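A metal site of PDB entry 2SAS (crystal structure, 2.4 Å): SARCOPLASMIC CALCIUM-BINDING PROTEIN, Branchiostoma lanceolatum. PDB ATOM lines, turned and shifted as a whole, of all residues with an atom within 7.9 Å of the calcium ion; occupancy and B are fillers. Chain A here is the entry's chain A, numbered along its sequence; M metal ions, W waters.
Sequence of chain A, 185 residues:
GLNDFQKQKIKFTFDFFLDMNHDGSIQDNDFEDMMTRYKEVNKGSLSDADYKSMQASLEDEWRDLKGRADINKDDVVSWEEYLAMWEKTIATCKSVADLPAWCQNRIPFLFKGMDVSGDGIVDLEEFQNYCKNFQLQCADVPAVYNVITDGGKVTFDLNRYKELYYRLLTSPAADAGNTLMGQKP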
ATOM      1  N   SER A  25      16.726   8.614  12.610  1.00  0.00           N
ATOM      2  CA  SER A  25      16.883   8.221  11.204  1.00  0.00           C
ATOM      3  C   SER A  25      17.592   9.407  10.474  1.00  0.00           C
ATOM      4  O   SER A  25      17.295  10.528  10.842  1.00  0.00           O
ATOM      5  CB  SER A  25      15.583   8.129  10.470  1.00  0.00           C
ATOM      6  OG  SER A  25      14.808   7.022  10.371  1.00  0.00           O
ATOM      7  N   ILE A  26      18.367   9.017   9.499  1.00  0.00           N
ATOM      8  CA  ILE A  26      19.074   9.865   8.586  1.00  0.00           C
ATOM      9  C   ILE A  26      18.128   9.870   7.336  1.00  0.00           C
ATOM     10  O   ILE A  26      17.742   8.768   6.945  1.00  0.00           O
ATOM     11  CB  ILE A  26      20.492   9.446   8.084  1.00  0.00           C
ATOM     12  CG1 ILE A  26      21.442   8.913   9.187  1.00  0.00           C
ATOM     13  CG2 ILE A  26      21.175  10.675   7.407  1.00  0.00           C
ATOM     14  CD1 ILE A  26      21.457   9.751  10.476  1.00  0.00           C
ATOM     15  N   TRP A  62      24.386  12.477   0.500  1.00  0.00           N
ATOM     16  CA  TRP A  62      23.209  11.672   0.839  1.00  0.00           C
ATOM     17  C   TRP A  62      23.087  10.442  -0.092  1.00  0.00           C
ATOM     18  O   TRP A  62      22.813   9.312   0.321  1.00  0.00           O
ATOM     19  CB  TRP A  62      21.938  12.508   0.738  1.00  0.00           C
ATOM     20  CG  TRP A  62      20.642  11.782   0.853  1.00  0.00           C
ATOM     21  CD1 TRP A  62      19.544  11.826   0.017  1.00  0.00           C
ATOM     22  CD2 TRP A  62      20.325  10.824   1.897  1.00  0.00           C
ATOM     23  NE1 TRP A  62      18.553  11.021   0.499  1.00  0.00           N
ATOM     24  CE2 TRP A  62      19.006  10.391   1.633  1.00  0.00           C
ATOM     25  CE3 TRP A  62      20.996  10.368   3.013  1.00  0.00           C
ATOM     26  CZ2 TRP A  62      18.368   9.489   2.500  1.00  0.00           C
ATOM     27  CZ3 TRP A  62      20.398   9.496   3.853  1.00  0.00           C
ATOM     28  CH2 TRP A  62      19.086   9.042   3.592  1.00  0.00           C
ATOM     29  N   LYS A  66      22.989   6.835   1.308  1.00  0.00           N
ATOM     30  CA  LYS A  66      21.760   6.094   0.986  1.00  0.00           C
ATOM     31  C   LYS A  66      22.080   4.827   0.196  1.00  0.00           C
ATOM     32  O   LYS A  66      21.583   3.726   0.516  1.00  0.00           O
ATOM     33  CB  LYS A  66      20.796   6.924   0.147  1.00  0.00           C
ATOM     34  CG  LYS A  66      19.323   6.678   0.261  1.00  0.00           C
ATOM     35  CD  LYS A  66      18.470   7.577  -0.619  1.00  0.00           C
ATOM     36  CE  LYS A  66      18.425   7.206  -2.076  1.00  0.00           C
ATOM     37  NZ  LYS A  66      19.660   7.621  -2.789  1.00  0.00           N
ATOM     38  N   ALA A  69      24.012   2.192   2.705  1.00  0.00           N
ATOM     39  CA  ALA A  69      23.445   1.773   3.988  1.00  0.00           C
ATOM     40  C   ALA A  69      21.977   1.472   3.932  1.00  0.00           C
ATOM     41  O   ALA A  69      21.545   0.752   4.829  1.00  0.00           O
ATOM     42  CB  ALA A  69      23.769   2.842   5.069  1.00  0.00           C
ATOM     43  N   ASP A  70      21.289   1.994   2.939  1.00  0.00           N
ATOM     44  CA  ASP A  70      19.843   1.716   2.881  1.00  0.00           C
ATOM     45  C   ASP A  70      19.608   0.324   2.228  1.00  0.00           C
ATOM     46  O   ASP A  70      19.333   0.232   1.021  1.00  0.00           O
ATOM     47  CB  ASP A  70      19.117   2.796   2.149  1.00  0.00           C
ATOM     48  CG  ASP A  70      17.604   2.755   2.343  1.00  0.00           C
ATOM     49  OD1 ASP A  70      17.095   2.298   3.402  1.00  0.00           O
ATOM     50  OD2 ASP A  70      17.035   3.278   1.378  1.00  0.00           O
ATOM     51  N   ILE A  71      19.647  -0.662   3.085  1.00  0.00           N
ATOM     52  CA  ILE A  71      19.470  -2.038   2.640  1.00  0.00           C
ATOM     53  C   ILE A  71      18.098  -2.348   2.061  1.00  0.00           C
ATOM     54  O   ILE A  71      18.115  -3.022   1.000  1.00  0.00           O
ATOM     55  CB  ILE A  71      19.941  -3.036   3.752  1.00  0.00           C
ATOM     56  CG1 ILE A  71      21.461  -2.817   4.047  1.00  0.00           C
ATOM     57  CG2 ILE A  71      19.673  -4.488   3.282  1.00  0.00           C
ATOM     58  CD1 ILE A  71      22.378  -2.875   2.772  1.00  0.00           C
ATOM     59  N   ASN A  72      16.984  -1.918   2.624  1.00  0.00           N
ATOM     60  CA  ASN A  72      15.644  -2.175   2.122  1.00  0.00           C
ATOM     61  C   ASN A  72      15.063  -1.077   1.224  1.00  0.00           C
ATOM     62  O   ASN A  72      13.809  -1.013   1.146  1.00  0.00           O
ATOM     63  CB  ASN A  72      14.580  -2.378   3.219  1.00  0.00           C
ATOM     64  CG  ASN A  72      14.415  -1.069   3.944  1.00  0.00           C
ATOM     65  OD1 ASN A  72      15.384  -0.311   3.855  1.00  0.00           O
ATOM     66  ND2 ASN A  72      13.392  -0.763   4.697  1.00  0.00           N
ATOM     67  N   LYS A  73      15.848  -0.251   0.624  1.00  0.00           N
ATOM     68  CA  LYS A  73      15.443   0.792  -0.265  1.00  0.00           C
ATOM     69  C   LYS A  73      14.280   1.701   0.025  1.00  0.00           C
ATOM     70  O   LYS A  73      13.597   2.074  -0.976  1.00  0.00           O
ATOM     71  CB  LYS A  73      15.183   0.136  -1.658  1.00  0.00           C
ATOM     72  CG  LYS A  73      16.460   0.300  -2.525  1.00  0.00           C
ATOM     73  CD  LYS A  73      17.599  -0.477  -1.873  1.00  0.00           C
ATOM     74  CE  LYS A  73      17.570  -1.909  -2.353  1.00  0.00           C
ATOM     75  NZ  LYS A  73      18.579  -2.049  -3.448  1.00  0.00           N
ATOM     76  N   ASP A  74      14.066   2.170   1.222  1.00  0.00           N
ATOM     77  CA  ASP A  74      13.046   3.111   1.626  1.00  0.00           C
ATOM     78  C   ASP A  74      13.581   4.536   1.883  1.00  0.00           C
ATOM     79  O   ASP A  74      12.960   5.214   2.736  1.00  0.00           O
ATOM     80  CB  ASP A  74      12.316   2.627   2.907  1.00  0.00           C
ATOM     81  CG  ASP A  74      13.131   2.516   4.156  1.00  0.00           C
ATOM     82  OD1 ASP A  74      14.383   2.474   4.049  1.00  0.00           O
ATOM     83  OD2 ASP A  74      12.628   2.465   5.301  1.00  0.00           O
ATOM     84  N   ASP A  75      14.650   4.988   1.307  1.00  0.00           N
ATOM     85  CA  ASP A  75      15.256   6.322   1.464  1.00  0.00           C
ATOM     86  C   ASP A  75      15.433   6.826   2.877  1.00  0.00           C
ATOM     87  O   ASP A  75      15.471   8.075   3.123  1.00  0.00           O
ATOM     88  CB  ASP A  75      14.427   7.388   0.668  1.00  0.00           C
ATOM     89  CG  ASP A  75      14.507   7.137  -0.813  1.00  0.00           C
ATOM     90  OD1 ASP A  75      15.565   6.706  -1.280  1.00  0.00           O
ATOM     91  OD2 ASP A  75      13.452   7.330  -1.481  1.00  0.00           O
ATOM     92  N   VAL A  76      15.488   5.956   3.826  1.00  0.00           N
ATOM     93  CA  VAL A  76      15.703   6.306   5.246  1.00  0.00           C
ATOM     94  C   VAL A  76      16.902   5.448   5.674  1.00  0.00           C
ATOM     95  O   VAL A  76      16.887   4.240   5.328  1.00  0.00           O
ATOM     96  CB  VAL A  76      14.468   6.009   6.087  1.00  0.00           C
ATOM     97  CG1 VAL A  76      14.638   6.478   7.542  1.00  0.00           C
ATOM     98  CG2 VAL A  76      13.176   6.545   5.493  1.00  0.00           C
ATOM     99  N   VAL A  77      17.912   6.038   6.306  1.00  0.00           N
ATOM    100  CA  VAL A  77      19.023   5.192   6.795  1.00  0.00           C
ATOM    101  C   VAL A  77      18.711   5.077   8.302  1.00  0.00           C
ATOM    102  O   VAL A  77      18.603   6.125   8.987  1.00  0.00           O
ATOM    103  CB  VAL A  77      20.409   5.697   6.481  1.00  0.00           C
ATOM    104  CG1 VAL A  77      21.504   4.935   7.234  1.00  0.00           C
ATOM    105  CG2 VAL A  77      20.758   5.723   4.990  1.00  0.00           C
ATOM    106  N   SER A  78      18.497   3.868   8.806  1.00  0.00           N
ATOM    107  CA  SER A  78      18.210   3.824  10.279  1.00  0.00           C
ATOM    108  C   SER A  78      19.551   3.640  10.978  1.00  0.00           C
ATOM    109  O   SER A  78      20.578   3.422  10.313  1.00  0.00           O
ATOM    110  CB  SER A  78      17.266   2.640  10.543  1.00  0.00           C
ATOM    111  OG  SER A  78      17.765   1.547   9.793  1.00  0.00           O
ATOM    112  N   GLU A  81      20.942   0.207  10.170  1.00  0.00           N
ATOM    113  CA  GLU A  81      21.644   0.116   8.882  1.00  0.00           C
ATOM    114  C   GLU A  81      22.953   0.903   8.912  1.00  0.00           C
ATOM    115  O   GLU A  81      23.949   0.465   8.300  1.00  0.00           O
ATOM    116  CB  GLU A  81      20.841   0.526   7.667  1.00  0.00           C
ATOM    117  CG  GLU A  81      19.349   0.093   7.743  1.00  0.00           C
ATOM    118  CD  GLU A  81      18.526   0.683   6.639  1.00  0.00           C
ATOM    119  OE1 GLU A  81      17.997   1.776   6.705  1.00  0.00           O
ATOM    120  OE2 GLU A  81      18.510  -0.055   5.651  1.00  0.00           O
HETATM  121 CA    CA M   1      16.286   2.006   5.136  1.00  0.00          CA
HETATM  122  O   HOH W   1      15.011   1.779   7.022  1.00  0.00           O
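OD2 of Asp 70 lies within hydrogen-bond range of N of Asp 75, 2.9 Å away. OG of Ser 78 lies close to N of Glu 81. The backbone NH (N) of Ile 71 is in hydrogen-bond range of the side-chain carboxylate (OE2) of Glu 81 (2.9 Å).
Five residues have an atom within 4 Å of the calcium ion: Asp 70, Asn 72, Asp 74, Val 76 and Glu 81. The nearest printed residue that does not touch the calcium ion is Val 77 (4.5 Å).
The calcium ion is bound by the side-chain carboxylate of Asp 70 (1.9 Å), the side-chain carboxylate of Asp 74 (2.2 Å), water W1 (2.3 Å), the backbone carbonyl oxygen of Val 76 (2.3 Å), the side-chain carboxylate of Glu 81 (2.3 Å) and the side-chain amide oxygen of Asn 72 (2.8 Å). The calcium ion has six donor atoms within binding distance. Slightly farther from the calcium ion lies the side-chain carboxylate (OE2) of Glu 81 (3.1 Å).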
